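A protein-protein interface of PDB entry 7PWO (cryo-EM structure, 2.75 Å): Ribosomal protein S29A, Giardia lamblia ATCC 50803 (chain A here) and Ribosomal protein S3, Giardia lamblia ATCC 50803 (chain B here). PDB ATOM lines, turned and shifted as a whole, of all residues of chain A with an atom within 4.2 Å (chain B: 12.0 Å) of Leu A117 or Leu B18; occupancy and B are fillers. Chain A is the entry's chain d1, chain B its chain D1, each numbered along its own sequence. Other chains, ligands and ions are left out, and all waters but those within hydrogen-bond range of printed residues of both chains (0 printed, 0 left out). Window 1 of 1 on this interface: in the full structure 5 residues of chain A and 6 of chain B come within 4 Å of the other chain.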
ATOM      1  N   ARG A 103      11.947 -20.078  13.170  1.00  0.00           N
ATOM      2  CA  ARG A 103      13.178 -20.788  12.858  1.00  0.00           C
ATOM      3  C   ARG A 103      13.132 -21.550  11.545  1.00  0.00           C
ATOM      4  O   ARG A 103      14.179 -22.004  11.078  1.00  0.00           O
ATOM      5  CB  ARG A 103      13.568 -21.740  13.992  1.00  0.00           C
ATOM      6  CG  ARG A 103      13.962 -21.030  15.248  1.00  0.00           C
ATOM      7  CD  ARG A 103      14.338 -21.977  16.373  1.00  0.00           C
ATOM      8  NE  ARG A 103      13.256 -22.766  16.923  1.00  0.00           N
ATOM      9  CZ  ARG A 103      13.448 -23.731  17.811  1.00  0.00           C
ATOM     10  NH1 ARG A 103      14.676 -24.033  18.206  1.00  0.00           N
ATOM     11  NH2 ARG A 103      12.416 -24.377  18.314  1.00  0.00           N
ATOM     12  N   TYR A 112       5.287 -18.642  18.043  1.00  0.00           N
ATOM     13  CA  TYR A 112       5.018 -19.298  19.314  1.00  0.00           C
ATOM     14  C   TYR A 112       6.314 -19.493  20.085  1.00  0.00           C
ATOM     15  O   TYR A 112       7.281 -20.040  19.552  1.00  0.00           O
ATOM     16  CB  TYR A 112       4.346 -20.652  19.109  1.00  0.00           C
ATOM     17  CG  TYR A 112       3.006 -20.607  18.427  1.00  0.00           C
ATOM     18  CD1 TYR A 112       1.999 -19.784  18.899  1.00  0.00           C
ATOM     19  CD2 TYR A 112       2.730 -21.426  17.345  1.00  0.00           C
ATOM     20  CE1 TYR A 112       0.772 -19.754  18.301  1.00  0.00           C
ATOM     21  CE2 TYR A 112       1.504 -21.404  16.746  1.00  0.00           C
ATOM     22  CZ  TYR A 112       0.527 -20.560  17.224  1.00  0.00           C
ATOM     23  OH  TYR A 112      -0.705 -20.524  16.629  1.00  0.00           O
ATOM     24  N   LYS A 114       5.863 -20.593  23.530  1.00  0.00           N
ATOM     25  CA  LYS A 114       5.525 -21.611  24.511  1.00  0.00           C
ATOM     26  C   LYS A 114       6.510 -22.760  24.388  1.00  0.00           C
ATOM     27  O   LYS A 114       6.896 -23.144  23.280  1.00  0.00           O
ATOM     28  CB  LYS A 114       4.103 -22.127  24.288  1.00  0.00           C
ATOM     29  CG  LYS A 114       3.628 -23.092  25.363  1.00  0.00           C
ATOM     30  CD  LYS A 114       2.208 -23.586  25.106  1.00  0.00           C
ATOM     31  CE  LYS A 114       1.157 -22.526  25.324  1.00  0.00           C
ATOM     32  NZ  LYS A 114       1.016 -22.102  26.737  1.00  0.00           N
ATOM     33  N   TYR A 115       6.967 -23.269  25.530  1.00  0.00           N
ATOM     34  CA  TYR A 115       7.812 -24.453  25.616  1.00  0.00           C
ATOM     35  C   TYR A 115       9.170 -24.215  24.967  1.00  0.00           C
ATOM     36  O   TYR A 115      10.026 -25.104  25.006  1.00  0.00           O
ATOM     37  CB  TYR A 115       7.141 -25.662  24.947  1.00  0.00           C
ATOM     38  CG  TYR A 115       5.845 -26.084  25.602  1.00  0.00           C
ATOM     39  CD1 TYR A 115       5.484 -25.624  26.860  1.00  0.00           C
ATOM     40  CD2 TYR A 115       4.911 -26.817  24.894  1.00  0.00           C
ATOM     41  CE1 TYR A 115       4.274 -25.979  27.427  1.00  0.00           C
ATOM     42  CE2 TYR A 115       3.697 -27.165  25.445  1.00  0.00           C
ATOM     43  CZ  TYR A 115       3.380 -26.748  26.705  1.00  0.00           C
ATOM     44  OH  TYR A 115       2.162 -27.105  27.238  1.00  0.00           O
ATOM     45  N   GLY A 116       9.284 -23.113  24.218  1.00  0.00           N
ATOM     46  CA  GLY A 116      10.511 -22.873  23.438  1.00  0.00           C
ATOM     47  C   GLY A 116      10.393 -23.466  22.040  1.00  0.00           C
ATOM     48  O   GLY A 116      11.372 -24.086  21.585  1.00  0.00           O
ATOM     49  N   LEU A 117       9.240 -23.295  21.378  1.00  0.00           N
ATOM     50  CA  LEU A 117       9.073 -23.801  19.985  1.00  0.00           C
ATOM     51  C   LEU A 117       9.700 -22.809  19.004  1.00  0.00           C
ATOM     52  O   LEU A 117      10.276 -23.265  17.997  1.00  0.00           O
ATOM     53  CB  LEU A 117       7.591 -24.031  19.679  1.00  0.00           C
ATOM     54  CG  LEU A 117       6.830 -24.848  20.720  1.00  0.00           C
ATOM     55  CD1 LEU A 117       5.443 -25.206  20.213  1.00  0.00           C
ATOM     56  CD2 LEU A 117       7.602 -26.103  21.097  1.00  0.00           C
ATOM     57  N   PHE A 118       9.588 -21.509  19.273  1.00  0.00           N
ATOM     58  CA  PHE A 118      10.302 -20.533  18.414  1.00  0.00           C
ATOM     59  C   PHE A 118       9.968 -20.772  16.938  1.00  0.00           C
ATOM     60  O   PHE A 118      10.909 -20.928  16.137  1.00  0.00           O
ATOM     61  CB  PHE A 118      11.804 -20.672  18.659  1.00  0.00           C
ATOM     62  CG  PHE A 118      12.193 -20.645  20.113  1.00  0.00           C
ATOM     63  CD1 PHE A 118      11.838 -19.576  20.919  1.00  0.00           C
ATOM     64  CD2 PHE A 118      12.912 -21.686  20.677  1.00  0.00           C
ATOM     65  CE1 PHE A 118      12.192 -19.549  22.258  1.00  0.00           C
ATOM     66  CE2 PHE A 118      13.269 -21.657  22.016  1.00  0.00           C
ATOM     67  CZ  PHE A 118      12.909 -20.589  22.803  1.00  0.00           C
ATOM     68  N   ILE A 119       8.676 -20.798  16.596  1.00  0.00           N
ATOM     69  CA  ILE A 119       8.234 -21.006  15.184  1.00  0.00           C
ATOM     70  C   ILE A 119       6.870 -20.336  15.025  1.00  0.00           C
ATOM     71  O   ILE A 119       6.320 -19.891  16.043  1.00  0.00           O
ATOM     72  CB  ILE A 119       8.172 -22.507  14.839  1.00  0.00           C
ATOM     73  CG1 ILE A 119       7.761 -23.348  16.050  1.00  0.00           C
ATOM     74  CG2 ILE A 119       9.489 -22.983  14.248  1.00  0.00           C
ATOM     75  CD1 ILE A 119       7.779 -24.837  15.800  1.00  0.00           C
ATOM     76  N   VAL B  12      11.676 -31.477  34.973  1.00  0.00           N
ATOM     77  CA  VAL B  12      11.784 -31.074  33.578  1.00  0.00           C
ATOM     78  C   VAL B  12      12.892 -31.833  32.843  1.00  0.00           C
ATOM     79  O   VAL B  12      14.048 -31.412  32.813  1.00  0.00           O
ATOM     80  CB  VAL B  12      12.017 -29.567  33.458  1.00  0.00           C
ATOM     81  CG1 VAL B  12      11.934 -29.149  32.009  1.00  0.00           C
ATOM     82  CG2 VAL B  12      11.001 -28.815  34.293  1.00  0.00           C
ATOM     83  N   TYR B  13      12.508 -32.949  32.228  1.00  0.00           N
ATOM     84  CA  TYR B  13      13.394 -33.766  31.413  1.00  0.00           C
ATOM     85  C   TYR B  13      13.027 -33.706  29.942  1.00  0.00           C
ATOM     86  O   TYR B  13      13.418 -34.594  29.174  1.00  0.00           O
ATOM     87  CB  TYR B  13      13.363 -35.218  31.888  1.00  0.00           C
ATOM     88  CG  TYR B  13      14.295 -35.502  33.029  1.00  0.00           C
ATOM     89  CD1 TYR B  13      15.609 -35.056  33.008  1.00  0.00           C
ATOM     90  CD2 TYR B  13      13.861 -36.213  34.129  1.00  0.00           C
ATOM     91  CE1 TYR B  13      16.466 -35.315  34.061  1.00  0.00           C
ATOM     92  CE2 TYR B  13      14.704 -36.473  35.185  1.00  0.00           C
ATOM     93  CZ  TYR B  13      16.005 -36.024  35.146  1.00  0.00           C
ATOM     94  OH  TYR B  13      16.834 -36.295  36.209  1.00  0.00           O
ATOM     95  N   TYR B  14      12.276 -32.676  29.537  1.00  0.00           N
ATOM     96  CA  TYR B  14      11.566 -32.710  28.272  1.00  0.00           C
ATOM     97  C   TYR B  14      12.052 -31.688  27.261  1.00  0.00           C
ATOM     98  O   TYR B  14      11.802 -31.864  26.066  1.00  0.00           O
ATOM     99  CB  TYR B  14      10.069 -32.509  28.523  1.00  0.00           C
ATOM    100  CG  TYR B  14       9.437 -33.814  28.889  1.00  0.00           C
ATOM    101  CD1 TYR B  14       9.689 -34.943  28.154  1.00  0.00           C
ATOM    102  CD2 TYR B  14       8.609 -33.928  29.976  1.00  0.00           C
ATOM    103  CE1 TYR B  14       9.122 -36.143  28.495  1.00  0.00           C
ATOM    104  CE2 TYR B  14       8.036 -35.115  30.304  1.00  0.00           C
ATOM    105  CZ  TYR B  14       8.295 -36.226  29.563  1.00  0.00           C
ATOM    106  OH  TYR B  14       7.732 -37.434  29.883  1.00  0.00           O
ATOM    107  N   SER B  15      12.730 -30.630  27.709  1.00  0.00           N
ATOM    108  CA  SER B  15      13.469 -29.770  26.795  1.00  0.00           C
ATOM    109  C   SER B  15      14.385 -30.587  25.894  1.00  0.00           C
ATOM    110  O   SER B  15      14.418 -30.398  24.671  1.00  0.00           O
ATOM    111  CB  SER B  15      14.283 -28.770  27.607  1.00  0.00           C
ATOM    112  OG  SER B  15      15.557 -29.322  27.915  1.00  0.00           O
ATOM    113  N   LYS B  16      15.146 -31.498  26.500  1.00  0.00           N
ATOM    114  CA  LYS B  16      16.067 -32.356  25.765  1.00  0.00           C
ATOM    115  C   LYS B  16      15.349 -33.104  24.648  1.00  0.00           C
ATOM    116  O   LYS B  16      15.768 -33.078  23.479  1.00  0.00           O
ATOM    117  CB  LYS B  16      16.712 -33.340  26.749  1.00  0.00           C
ATOM    118  CG  LYS B  16      17.909 -32.791  27.531  1.00  0.00           C
ATOM    119  CD  LYS B  16      17.494 -31.800  28.607  1.00  0.00           C
ATOM    120  CE  LYS B  16      16.739 -32.452  29.742  1.00  0.00           C
ATOM    121  NZ  LYS B  16      16.376 -31.516  30.835  1.00  0.00           N
ATOM    122  N   TYR B  17      14.226 -33.734  24.984  1.00  0.00           N
ATOM    123  CA  TYR B  17      13.574 -34.608  24.022  1.00  0.00           C
ATOM    124  C   TYR B  17      12.898 -33.779  22.936  1.00  0.00           C
ATOM    125  O   TYR B  17      12.902 -34.157  21.760  1.00  0.00           O
ATOM    126  CB  TYR B  17      12.521 -35.465  24.716  1.00  0.00           C
ATOM    127  CG  TYR B  17      11.932 -36.525  23.820  1.00  0.00           C
ATOM    128  CD1 TYR B  17      12.641 -37.695  23.600  1.00  0.00           C
ATOM    129  CD2 TYR B  17      10.777 -36.321  23.085  1.00  0.00           C
ATOM    130  CE1 TYR B  17      12.161 -38.691  22.797  1.00  0.00           C
ATOM    131  CE2 TYR B  17      10.283 -37.328  22.242  1.00  0.00           C
ATOM    132  CZ  TYR B  17      10.997 -38.512  22.105  1.00  0.00           C
ATOM    133  OH  TYR B  17      10.575 -39.538  21.289  1.00  0.00           O
ATOM    134  N   LEU B  18      12.291 -32.655  23.327  1.00  0.00           N
ATOM    135  CA  LEU B  18      11.623 -31.774  22.371  1.00  0.00           C
ATOM    136  C   LEU B  18      12.607 -31.209  21.356  1.00  0.00           C
ATOM    137  O   LEU B  18      12.302 -31.129  20.156  1.00  0.00           O
ATOM    138  CB  LEU B  18      10.922 -30.644  23.128  1.00  0.00           C
ATOM    139  CG  LEU B  18       9.956 -29.727  22.379  1.00  0.00           C
ATOM    140  CD1 LEU B  18       8.579 -30.353  22.305  1.00  0.00           C
ATOM    141  CD2 LEU B  18       9.898 -28.362  23.046  1.00  0.00           C
ATOM    142  N   ASN B  19      13.788 -30.793  21.819  1.00  0.00           N
ATOM    143  CA  ASN B  19      14.818 -30.361  20.885  1.00  0.00           C
ATOM    144  C   ASN B  19      15.280 -31.512  19.998  1.00  0.00           C
ATOM    145  O   ASN B  19      15.590 -31.296  18.821  1.00  0.00           O
ATOM    146  CB  ASN B  19      15.993 -29.744  21.646  1.00  0.00           C
ATOM    147  CG  ASN B  19      15.611 -28.472  22.359  1.00  0.00           C
ATOM    148  OD1 ASN B  19      14.434 -28.234  22.636  1.00  0.00           O
ATOM    149  ND2 ASN B  19      16.599 -27.638  22.661  1.00  0.00           N
ATOM    150  N   ASP B  20      15.316 -32.738  20.524  1.00  0.00           N
ATOM    151  CA  ASP B  20      15.567 -33.872  19.633  1.00  0.00           C
ATOM    152  C   ASP B  20      14.513 -33.966  18.536  1.00  0.00           C
ATOM    153  O   ASP B  20      14.847 -34.222  17.375  1.00  0.00           O
ATOM    154  CB  ASP B  20      15.662 -35.186  20.413  1.00  0.00           C
ATOM    155  CG  ASP B  20      16.916 -35.268  21.267  1.00  0.00           C
ATOM    156  OD1 ASP B  20      17.922 -34.651  20.875  1.00  0.00           O
ATOM    157  OD2 ASP B  20      16.928 -35.977  22.290  1.00  0.00           O
ATOM    158  N   CYS B  21      13.240 -33.770  18.880  1.00  0.00           N
ATOM    159  CA  CYS B  21      12.192 -33.807  17.859  1.00  0.00           C
ATOM    160  C   CYS B  21      12.391 -32.716  16.809  1.00  0.00           C
ATOM    161  O   CYS B  21      12.299 -32.978  15.601  1.00  0.00           O
ATOM    162  CB  CYS B  21      10.803 -33.674  18.490  1.00  0.00           C
ATOM    163  SG  CYS B  21      10.390 -34.762  19.867  1.00  0.00           S
ATOM    164  N   ILE B  22      12.670 -31.484  17.243  1.00  0.00           N
ATOM    165  CA  ILE B  22      12.775 -30.401  16.263  1.00  0.00           C
ATOM    166  C   ILE B  22      14.009 -30.589  15.383  1.00  0.00           C
ATOM    167  O   ILE B  22      13.998 -30.243  14.195  1.00  0.00           O
ATOM    168  CB  ILE B  22      12.754 -29.012  16.927  1.00  0.00           C
ATOM    169  CG1 ILE B  22      12.598 -27.959  15.834  1.00  0.00           C
ATOM    170  CG2 ILE B  22      14.036 -28.725  17.688  1.00  0.00           C
ATOM    171  CD1 ILE B  22      12.258 -26.621  16.320  1.00  0.00           C
ATOM    172  N   MET B  23      15.082 -31.167  15.931  1.00  0.00           N
ATOM    173  CA  MET B  23      16.256 -31.446  15.109  1.00  0.00           C
ATOM    174  C   MET B  23      16.047 -32.646  14.185  1.00  0.00           C
ATOM    175  O   MET B  23      16.635 -32.693  13.101  1.00  0.00           O
ATOM    176  CB  MET B  23      17.481 -31.656  16.001  1.00  0.00           C
ATOM    177  CG  MET B  23      17.631 -33.054  16.567  1.00  0.00           C
ATOM    178  SD  MET B  23      19.242 -33.329  17.326  1.00  0.00           S
ATOM    179  CE  MET B  23      20.340 -32.872  15.992  1.00  0.00           C
ATOM    180  N   GLU B  24      15.223 -33.621  14.576  1.00  0.00           N
ATOM    181  CA  GLU B  24      14.853 -34.667  13.630  1.00  0.00           C
ATOM    182  C   GLU B  24      14.064 -34.081  12.465  1.00  0.00           C
ATOM    183  O   GLU B  24      14.249 -34.497  11.308  1.00  0.00           O
ATOM    184  CB  GLU B  24      14.057 -35.758  14.351  1.00  0.00           C
ATOM    185  CG  GLU B  24      14.069 -37.110  13.663  1.00  0.00           C
ATOM    186  CD  GLU B  24      13.153 -37.180  12.459  1.00  0.00           C
ATOM    187  OE1 GLU B  24      11.963 -36.838  12.599  1.00  0.00           O
ATOM    188  OE2 GLU B  24      13.621 -37.560  11.366  1.00  0.00           O
ATOM    189  N   ALA B  25      13.212 -33.089  12.752  1.00  0.00           N
ATOM    190  CA  ALA B  25      12.518 -32.368  11.683  1.00  0.00           C
ATOM    191  C   ALA B  25      13.509 -31.653  10.772  1.00  0.00           C
ATOM    192  O   ALA B  25      13.413 -31.737   9.539  1.00  0.00           O
ATOM    193  CB  ALA B  25      11.520 -31.377  12.277  1.00  0.00           C
ATOM    194  N   GLU B  26      14.458 -30.925  11.368  1.00  0.00           N
ATOM    195  CA  GLU B  26      15.615 -30.400  10.645  1.00  0.00           C
ATOM    196  C   GLU B  26      16.253 -31.389   9.679  1.00  0.00           C
ATOM    197  O   GLU B  26      16.432 -31.092   8.492  1.00  0.00           O
ATOM    198  CB  GLU B  26      16.667 -29.917  11.642  1.00  0.00           C
ATOM    199  CG  GLU B  26      17.901 -29.349  10.960  1.00  0.00           C
ATOM    200  CD  GLU B  26      17.630 -28.106  10.160  1.00  0.00           C
ATOM    201  OE1 GLU B  26      16.667 -27.385  10.473  1.00  0.00           O
ATOM    202  OE2 GLU B  26      18.378 -27.872   9.189  1.00  0.00           O
ATOM    203  N   LEU B  27      16.668 -32.546  10.191  1.00  0.00           N
ATOM    204  CA  LEU B  27      17.415 -33.461   9.341  1.00  0.00           C
ATOM    205  C   LEU B  27      16.550 -33.996   8.207  1.00  0.00           C
ATOM    206  O   LEU B  27      17.020 -34.096   7.068  1.00  0.00           O
ATOM    207  CB  LEU B  27      18.030 -34.594  10.162  1.00  0.00           C
ATOM    208  CG  LEU B  27      18.683 -34.218  11.489  1.00  0.00           C
ATOM    209  CD1 LEU B  27      18.821 -35.441  12.383  1.00  0.00           C
ATOM    210  CD2 LEU B  27      20.044 -33.553  11.255  1.00  0.00           C
ATOM    211  N   LEU B  45      16.065 -40.860  14.374  1.00  0.00           N
ATOM    212  CA  LEU B  45      17.075 -40.261  15.239  1.00  0.00           C
ATOM    213  C   LEU B  45      17.252 -41.095  16.501  1.00  0.00           C
ATOM    214  O   LEU B  45      16.272 -41.436  17.166  1.00  0.00           O
ATOM    215  CB  LEU B  45      16.687 -38.815  15.571  1.00  0.00           C
ATOM    216  CG  LEU B  45      17.549 -37.962  16.491  1.00  0.00           C
ATOM    217  CD1 LEU B  45      17.626 -36.547  15.942  1.00  0.00           C
ATOM    218  CD2 LEU B  45      16.930 -37.939  17.867  1.00  0.00           C
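Of chain B, only Leu B18 comes within 4 Å of Leu A117. Leu B18 touches just these residues of chain A: Tyr A115 (3.8 Å) and Leu A117 (3.8 Å). No residue of chain B comes within 4 Å of Gly A116. No residue of chain B comes within 4 Å of Phe A118. No residue of chain B comes within 4 Å of Ile A119. Of the printed residues of chain A, Ile B22 touches Arg A103. Printed residues of chain B within 4 Å of Tyr A115: Leu B18 (3.8 Å). The nearest printed residue of chain A that does not touch Leu B18 is Gly A116 (4.8 Å).
Printed residues of chain A that touch a printed residue of chain B: Arg A103, Tyr A115 and Leu A117. Of the 17 printed residues of chain B, 2 touch a printed residue of chain A. Hydrophobic or aromatic side chains of chain B within 4 Å of the printed part of chain A: Leu B18 and Ile B22. Among the printed residues, 3 pairs touch across the chains. Among the printed residues, no Asp or Glu carboxylate lies within 4 Å of a Lys or Arg side-chain nitrogen of the other chain.
The backbone carbonyl oxygen (O) of Phe A118 sits close to the guanidinium group (NE) of Arg A103 (3.1 Å). The guanidinium group (NH2) of Arg A103 lies within hydrogen-bond range of the backbone carbonyl oxygen (O) of Leu A117 (2.4 Å). The guanidinium group (NH2) of Arg A103 lies within hydrogen-bond range of the backbone carbonyl oxygen (O) of Gly A116 (3.4 Å).
NH2 of Arg A103 touches CD1 of Ile B22 (3.0 Å). Leu B18 touches Tyr A115. Leu A117 touches Leu B18.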
